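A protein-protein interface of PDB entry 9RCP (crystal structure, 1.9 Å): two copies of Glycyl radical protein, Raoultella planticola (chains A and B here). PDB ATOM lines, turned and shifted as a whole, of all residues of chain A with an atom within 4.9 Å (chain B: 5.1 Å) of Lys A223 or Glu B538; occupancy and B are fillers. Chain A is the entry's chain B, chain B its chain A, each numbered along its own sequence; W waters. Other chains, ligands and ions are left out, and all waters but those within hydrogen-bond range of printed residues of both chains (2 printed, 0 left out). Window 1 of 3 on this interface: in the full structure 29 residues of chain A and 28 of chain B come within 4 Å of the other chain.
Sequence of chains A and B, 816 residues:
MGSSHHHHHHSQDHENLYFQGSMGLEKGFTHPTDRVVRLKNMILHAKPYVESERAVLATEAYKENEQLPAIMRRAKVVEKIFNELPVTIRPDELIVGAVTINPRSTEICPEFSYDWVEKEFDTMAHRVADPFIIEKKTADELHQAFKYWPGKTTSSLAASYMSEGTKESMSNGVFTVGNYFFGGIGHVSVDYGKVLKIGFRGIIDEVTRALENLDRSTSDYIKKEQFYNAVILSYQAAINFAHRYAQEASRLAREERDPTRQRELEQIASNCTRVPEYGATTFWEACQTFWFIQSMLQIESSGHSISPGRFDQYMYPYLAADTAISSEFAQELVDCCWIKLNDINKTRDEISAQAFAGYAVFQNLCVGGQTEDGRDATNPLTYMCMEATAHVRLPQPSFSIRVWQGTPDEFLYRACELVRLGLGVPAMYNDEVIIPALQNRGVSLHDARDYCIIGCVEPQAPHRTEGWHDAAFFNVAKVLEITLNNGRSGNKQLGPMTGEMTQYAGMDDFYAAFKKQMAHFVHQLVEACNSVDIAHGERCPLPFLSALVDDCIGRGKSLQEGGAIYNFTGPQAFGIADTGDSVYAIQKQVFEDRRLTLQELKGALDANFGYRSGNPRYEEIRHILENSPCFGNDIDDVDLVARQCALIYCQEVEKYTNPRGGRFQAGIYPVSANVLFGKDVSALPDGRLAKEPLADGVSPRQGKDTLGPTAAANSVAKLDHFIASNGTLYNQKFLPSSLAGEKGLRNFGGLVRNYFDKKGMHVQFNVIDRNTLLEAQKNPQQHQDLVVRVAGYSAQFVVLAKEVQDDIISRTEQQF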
ATOM      1  N   SER A 219     -27.184  12.494  17.489  1.00  0.00           N
ATOM      2  CA  SER A 219     -26.680  13.659  18.213  1.00  0.00           C
ATOM      3  C   SER A 219     -27.682  14.810  18.294  1.00  0.00           C
ATOM      4  O   SER A 219     -27.446  15.766  19.051  1.00  0.00           O
ATOM      5  CB  SER A 219     -25.372  14.163  17.577  1.00  0.00           C
ATOM      6  OG  SER A 219     -25.603  14.629  16.260  1.00  0.00           O
ATOM      7  N   ASP A 220     -28.809  14.736  17.577  1.00  0.00           N
ATOM      8  CA  ASP A 220     -29.767  15.835  17.462  1.00  0.00           C
ATOM      9  C   ASP A 220     -30.437  16.178  18.785  1.00  0.00           C
ATOM     10  O   ASP A 220     -30.946  17.288  18.945  1.00  0.00           O
ATOM     11  CB  ASP A 220     -30.851  15.476  16.434  1.00  0.00           C
ATOM     12  CG  ASP A 220     -30.380  15.634  14.998  1.00  0.00           C
ATOM     13  OD1 ASP A 220     -29.295  16.198  14.775  1.00  0.00           O
ATOM     14  OD2 ASP A 220     -31.106  15.188  14.087  1.00  0.00           O
ATOM     15  N   TYR A 221     -30.500  15.218  19.716  1.00  0.00           N
ATOM     16  CA  TYR A 221     -31.207  15.434  20.984  1.00  0.00           C
ATOM     17  C   TYR A 221     -30.482  16.394  21.915  1.00  0.00           C
ATOM     18  O   TYR A 221     -31.118  16.996  22.786  1.00  0.00           O
ATOM     19  CB  TYR A 221     -31.436  14.074  21.666  1.00  0.00           C
ATOM     20  CG  TYR A 221     -30.285  13.569  22.525  1.00  0.00           C
ATOM     21  CD1 TYR A 221     -30.099  14.000  23.846  1.00  0.00           C
ATOM     22  CD2 TYR A 221     -29.391  12.624  22.010  1.00  0.00           C
ATOM     23  CE1 TYR A 221     -29.048  13.529  24.607  1.00  0.00           C
ATOM     24  CE2 TYR A 221     -28.358  12.144  22.756  1.00  0.00           C
ATOM     25  CZ  TYR A 221     -28.173  12.594  24.039  1.00  0.00           C
ATOM     26  OH  TYR A 221     -27.127  12.097  24.768  1.00  0.00           O
ATOM     27  N   ILE A 222     -29.170  16.573  21.734  1.00  0.00           N
ATOM     28  CA  ILE A 222     -28.391  17.378  22.677  1.00  0.00           C
ATOM     29  C   ILE A 222     -28.863  18.834  22.684  1.00  0.00           C
ATOM     30  O   ILE A 222     -29.136  19.413  23.749  1.00  0.00           O
ATOM     31  CB  ILE A 222     -26.895  17.262  22.353  1.00  0.00           C
ATOM     32  CG1 ILE A 222     -26.420  15.838  22.642  1.00  0.00           C
ATOM     33  CG2 ILE A 222     -26.078  18.243  23.186  1.00  0.00           C
ATOM     34  CD1 ILE A 222     -25.029  15.514  22.009  1.00  0.00           C
ATOM     35  N   LYS A 223     -28.972  19.456  21.498  1.00  0.00           N
ATOM     36  CA  LYS A 223     -29.413  20.853  21.468  1.00  0.00           C
ATOM     37  C   LYS A 223     -30.902  20.976  21.789  1.00  0.00           C
ATOM     38  O   LYS A 223     -31.333  21.995  22.343  1.00  0.00           O
ATOM     39  CB  LYS A 223     -29.092  21.504  20.117  1.00  0.00           C
ATOM     40  CG  LYS A 223     -27.588  21.806  19.951  1.00  0.00           C
ATOM     41  CD  LYS A 223     -27.241  22.424  18.586  1.00  0.00           C
ATOM     42  CE  LYS A 223     -27.710  23.872  18.495  1.00  0.00           C
ATOM     43  NZ  LYS A 223     -26.962  24.779  19.426  1.00  0.00           N
ATOM     44  N   LYS A 224     -31.700  19.968  21.439  1.00  0.00           N
ATOM     45  CA  LYS A 224     -33.125  20.038  21.753  1.00  0.00           C
ATOM     46  C   LYS A 224     -33.336  20.056  23.256  1.00  0.00           C
ATOM     47  O   LYS A 224     -34.172  20.808  23.780  1.00  0.00           O
ATOM     48  CB  LYS A 224     -33.859  18.864  21.122  1.00  0.00           C
ATOM     49  CG  LYS A 224     -33.896  18.873  19.604  1.00  0.00           C
ATOM     50  CD  LYS A 224     -34.757  17.720  19.107  1.00  0.00           C
ATOM     51  CE  LYS A 224     -34.841  17.685  17.597  1.00  0.00           C
ATOM     52  NZ  LYS A 224     -35.684  16.540  17.153  1.00  0.00           N
ATOM     53  N   GLU A 225     -32.548  19.260  23.971  1.00  0.00           N
ATOM     54  CA  GLU A 225     -32.661  19.188  25.417  1.00  0.00           C
ATOM     55  C   GLU A 225     -32.168  20.478  26.075  1.00  0.00           C
ATOM     56  O   GLU A 225     -32.740  20.912  27.084  1.00  0.00           O
ATOM     57  CB  GLU A 225     -31.919  17.920  25.858  1.00  0.00           C
ATOM     58  CG  GLU A 225     -31.362  17.810  27.245  1.00  0.00           C
ATOM     59  CD  GLU A 225     -30.973  16.355  27.545  1.00  0.00           C
ATOM     60  OE1 GLU A 225     -31.785  15.442  27.282  1.00  0.00           O
ATOM     61  OE2 GLU A 225     -29.815  16.120  27.945  1.00  0.00           O
ATOM     62  N   GLN A 226     -31.169  21.154  25.480  1.00  0.00           N
ATOM     63  CA  GLN A 226     -30.800  22.491  25.950  1.00  0.00           C
ATOM     64  C   GLN A 226     -31.977  23.451  25.834  1.00  0.00           C
ATOM     65  O   GLN A 226     -32.267  24.218  26.760  1.00  0.00           O
ATOM     66  CB  GLN A 226     -29.610  23.053  25.160  1.00  0.00           C
ATOM     67  CG  GLN A 226     -28.292  22.462  25.525  1.00  0.00           C
ATOM     68  CD  GLN A 226     -27.846  22.863  26.910  1.00  0.00           C
ATOM     69  OE1 GLN A 226     -27.921  24.035  27.308  1.00  0.00           O
ATOM     70  NE2 GLN A 226     -27.390  21.883  27.665  1.00  0.00           N
ATOM     71  N   PHE A 227     -32.646  23.433  24.680  1.00  0.00           N
ATOM     72  CA  PHE A 227     -33.823  24.267  24.472  1.00  0.00           C
ATOM     73  C   PHE A 227     -34.909  23.938  25.492  1.00  0.00           C
ATOM     74  O   PHE A 227     -35.482  24.835  26.124  1.00  0.00           O
ATOM     75  CB  PHE A 227     -34.348  24.076  23.047  1.00  0.00           C
ATOM     76  CG  PHE A 227     -35.646  24.772  22.798  1.00  0.00           C
ATOM     77  CD1 PHE A 227     -35.681  26.139  22.551  1.00  0.00           C
ATOM     78  CD2 PHE A 227     -36.837  24.073  22.831  1.00  0.00           C
ATOM     79  CE1 PHE A 227     -36.884  26.784  22.361  1.00  0.00           C
ATOM     80  CE2 PHE A 227     -38.036  24.710  22.625  1.00  0.00           C
ATOM     81  CZ  PHE A 227     -38.064  26.062  22.389  1.00  0.00           C
ATOM     82  N   GLY A 556     -38.660  21.074  19.488  1.00  0.00           N
ATOM     83  CA  GLY A 556     -37.492  21.367  20.298  1.00  0.00           C
ATOM     84  C   GLY A 556     -36.583  22.427  19.721  1.00  0.00           C
ATOM     85  O   GLY A 556     -35.358  22.329  19.869  1.00  0.00           O
ATOM     86  N   ALA B  70     -17.719  33.163  14.085  1.00  0.00           N
ATOM     87  CA  ALA B  70     -16.572  32.396  14.582  1.00  0.00           C
ATOM     88  C   ALA B  70     -15.508  32.123  13.513  1.00  0.00           C
ATOM     89  O   ALA B  70     -14.306  32.250  13.782  1.00  0.00           O
ATOM     90  CB  ALA B  70     -17.045  31.074  15.186  1.00  0.00           C
ATOM     91  N   LEU B 157     -18.018  25.490  27.075  1.00  0.00           N
ATOM     92  CA  LEU B 157     -19.266  25.274  26.348  1.00  0.00           C
ATOM     93  C   LEU B 157     -19.584  23.787  26.225  1.00  0.00           C
ATOM     94  O   LEU B 157     -20.740  23.378  26.415  1.00  0.00           O
ATOM     95  CB  LEU B 157     -19.184  25.926  24.960  1.00  0.00           C
ATOM     96  CG  LEU B 157     -20.395  25.699  24.039  1.00  0.00           C
ATOM     97  CD1 LEU B 157     -21.656  26.348  24.601  1.00  0.00           C
ATOM     98  CD2 LEU B 157     -20.124  26.191  22.602  1.00  0.00           C
ATOM     99  N   TYR B 161     -23.095  21.420  27.631  1.00  0.00           N
ATOM    100  CA  TYR B 161     -24.003  20.578  26.854  1.00  0.00           C
ATOM    101  C   TYR B 161     -24.204  19.179  27.437  1.00  0.00           C
ATOM    102  O   TYR B 161     -25.105  18.464  26.987  1.00  0.00           O
ATOM    103  CB  TYR B 161     -23.497  20.423  25.421  1.00  0.00           C
ATOM    104  CG  TYR B 161     -23.890  21.538  24.472  1.00  0.00           C
ATOM    105  CD1 TYR B 161     -25.229  21.747  24.123  1.00  0.00           C
ATOM    106  CD2 TYR B 161     -22.923  22.340  23.878  1.00  0.00           C
ATOM    107  CE1 TYR B 161     -25.581  22.751  23.236  1.00  0.00           C
ATOM    108  CE2 TYR B 161     -23.271  23.343  22.976  1.00  0.00           C
ATOM    109  CZ  TYR B 161     -24.590  23.543  22.659  1.00  0.00           C
ATOM    110  OH  TYR B 161     -24.925  24.539  21.769  1.00  0.00           O
ATOM    111  N   ILE B 534     -19.931  19.554  19.109  1.00  0.00           N
ATOM    112  CA  ILE B 534     -20.750  20.749  18.919  1.00  0.00           C
ATOM    113  C   ILE B 534     -19.987  21.992  19.354  1.00  0.00           C
ATOM    114  O   ILE B 534     -19.986  23.009  18.649  1.00  0.00           O
ATOM    115  CB  ILE B 534     -22.083  20.622  19.676  1.00  0.00           C
ATOM    116  CG1 ILE B 534     -22.963  19.531  19.053  1.00  0.00           C
ATOM    117  CG2 ILE B 534     -22.821  21.966  19.682  1.00  0.00           C
ATOM    118  CD1 ILE B 534     -24.087  19.098  19.960  1.00  0.00           C
ATOM    119  N   ALA B 535     -19.301  21.925  20.504  1.00  0.00           N
ATOM    120  CA  ALA B 535     -18.594  23.098  21.028  1.00  0.00           C
ATOM    121  C   ALA B 535     -17.499  23.592  20.073  1.00  0.00           C
ATOM    122  O   ALA B 535     -17.336  24.801  19.873  1.00  0.00           O
ATOM    123  CB  ALA B 535     -18.005  22.785  22.404  1.00  0.00           C
ATOM    124  N   HIS B 536     -16.723  22.676  19.493  1.00  0.00           N
ATOM    125  CA  HIS B 536     -15.714  23.089  18.518  1.00  0.00           C
ATOM    126  C   HIS B 536     -16.353  23.706  17.276  1.00  0.00           C
ATOM    127  O   HIS B 536     -15.816  24.664  16.704  1.00  0.00           O
ATOM    128  CB  HIS B 536     -14.850  21.901  18.139  1.00  0.00           C
ATOM    129  CG  HIS B 536     -13.736  21.650  19.100  1.00  0.00           C
ATOM    130  ND1 HIS B 536     -12.513  22.283  19.002  1.00  0.00           N
ATOM    131  CD2 HIS B 536     -13.664  20.856  20.196  1.00  0.00           C
ATOM    132  CE1 HIS B 536     -11.731  21.870  19.984  1.00  0.00           C
ATOM    133  NE2 HIS B 536     -12.406  21.006  20.724  1.00  0.00           N
ATOM    134  N   GLY B 537     -17.494  23.162  16.840  1.00  0.00           N
ATOM    135  CA  GLY B 537     -18.192  23.741  15.705  1.00  0.00           C
ATOM    136  C   GLY B 537     -18.704  25.144  15.973  1.00  0.00           C
ATOM    137  O   GLY B 537     -18.578  26.026  15.125  1.00  0.00           O
ATOM    138  N   GLU B 538     -19.283  25.375  17.156  1.00  0.00           N
ATOM    139  CA  GLU B 538     -19.850  26.690  17.440  1.00  0.00           C
ATOM    140  C   GLU B 538     -18.773  27.719  17.702  1.00  0.00           C
ATOM    141  O   GLU B 538     -18.950  28.892  17.367  1.00  0.00           O
ATOM    142  CB  GLU B 538     -20.799  26.658  18.644  1.00  0.00           C
ATOM    143  CG  GLU B 538     -21.689  25.429  18.748  1.00  0.00           C
ATOM    144  CD  GLU B 538     -22.963  25.669  19.568  1.00  0.00           C
ATOM    145  OE1 GLU B 538     -22.851  26.162  20.712  1.00  0.00           O
ATOM    146  OE2 GLU B 538     -24.057  25.288  19.081  1.00  0.00           O
ATOM    147  N   ARG B 539     -17.663  27.318  18.313  1.00  0.00           N
ATOM    148  CA  ARG B 539     -16.717  28.295  18.815  1.00  0.00           C
ATOM    149  C   ARG B 539     -15.364  28.295  18.116  1.00  0.00           C
ATOM    150  O   ARG B 539     -14.702  29.333  18.132  1.00  0.00           O
ATOM    151  CB  ARG B 539     -16.507  28.098  20.325  1.00  0.00           C
ATOM    152  CG  ARG B 539     -17.672  28.659  21.130  1.00  0.00           C
ATOM    153  CD  ARG B 539     -17.407  28.726  22.635  1.00  0.00           C
ATOM    154  NE  ARG B 539     -18.514  29.432  23.277  1.00  0.00           N
ATOM    155  CZ  ARG B 539     -18.574  29.757  24.562  1.00  0.00           C
ATOM    156  NH1 ARG B 539     -17.587  29.423  25.392  1.00  0.00           N
ATOM    157  NH2 ARG B 539     -19.632  30.430  25.012  1.00  0.00           N
ATOM    158  N   CYS B 540     -14.920  27.187  17.522  1.00  0.00           N
ATOM    159  CA  CYS B 540     -13.565  27.150  16.963  1.00  0.00           C
ATOM    160  C   CYS B 540     -13.490  26.374  15.640  1.00  0.00           C
ATOM    161  O   CYS B 540     -12.670  25.453  15.483  1.00  0.00           O
ATOM    162  CB  CYS B 540     -12.607  26.566  17.996  1.00  0.00           C
ATOM    163  SG  CYS B 540     -10.879  27.060  17.660  1.00  0.00           S
ATOM    164  N   PRO B 541     -14.274  26.772  14.631  1.00  0.00           N
ATOM    165  CA  PRO B 541     -14.046  26.222  13.294  1.00  0.00           C
ATOM    166  C   PRO B 541     -12.768  26.820  12.685  1.00  0.00           C
ATOM    167  O   PRO B 541     -12.448  27.989  12.898  1.00  0.00           O
ATOM    168  CB  PRO B 541     -15.313  26.635  12.535  1.00  0.00           C
ATOM    169  CG  PRO B 541     -15.675  27.958  13.131  1.00  0.00           C
ATOM    170  CD  PRO B 541     -15.317  27.821  14.610  1.00  0.00           C
HETATM  171  O   HOH W   1     -28.235  24.853  22.142  1.00  0.00           O
HETATM  172  O   HOH W   2     -27.692  19.437  26.277  1.00  0.00           O
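The side-chain hydroxyl of Tyr B161 is in hydrogen-bond range of the side-chain carboxylate of Glu B538, at 2.8 Å.
No position is printed for both chains. Of the 5 pairs that touch across the chains among the printed residues, none has its exchanged pair printed and touching as well.
Ile A222 touches Tyr B161. CG2 of Ile A222 touches CD1 of Ile B534, 3.9 Å away. CG of Gln A226 touches CD1 of Tyr B161, at 3.4 Å.
OH of Tyr B161 sits at hydrogen-bond distance from NZ of Lys A223, 3.1 Å away. OE2 of Glu B538 lies within salt-bridge range of NZ of Lys A223 (3.0 Å).
Of the 10 printed residues of chain A, 3 touch a printed residue of chain B. Printed residues of chain A that touch a printed residue of chain B: Ile A222, Lys A223 and Gln A226. Hydrophobic or aromatic side chains of chain A that line the printed part of chain B: Ile A222. Of the 11 printed residues of chain B, 3 touch a printed residue of chain A. Printed residues of chain B that touch a printed residue of chain A: Tyr B161, Ile B534 and Glu B538. Among the printed residues, 5 pairs touch across the chains.
Water W2 lies within hydrogen-bond range of the side-chain amide nitrogen (NE2) of Gln A226, the backbone carbonyl oxygen (O) of Tyr B161 and the backbone carbonyl oxygen (O) of Ile A222. Water W1 lies within hydrogen-bond range of the side-chain amino group of Lys A223 (3.0 Å) and the side-chain hydroxyl of Tyr B161 (3.3 Å).
Of the printed residues of chain B, Lys A223 touches Tyr B161 (3.1 Å) and Glu B538 (3.0 Å). Glu B538 touches one residue of chain A. Of the printed residues of chain A, Tyr B161 touches Ile A222, Lys A223 and Gln A226. Of the printed residues of chain A, Ile B534 touches Ile A222 (3.9 Å). Printed residues of chain B within 4 Å of Gln A226: Tyr B161 (3.4 Å). Of the printed residues of chain B, Ile A222 touches Tyr B161 and Ile B534. Lys A224 touches none of the printed residues of chain B.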
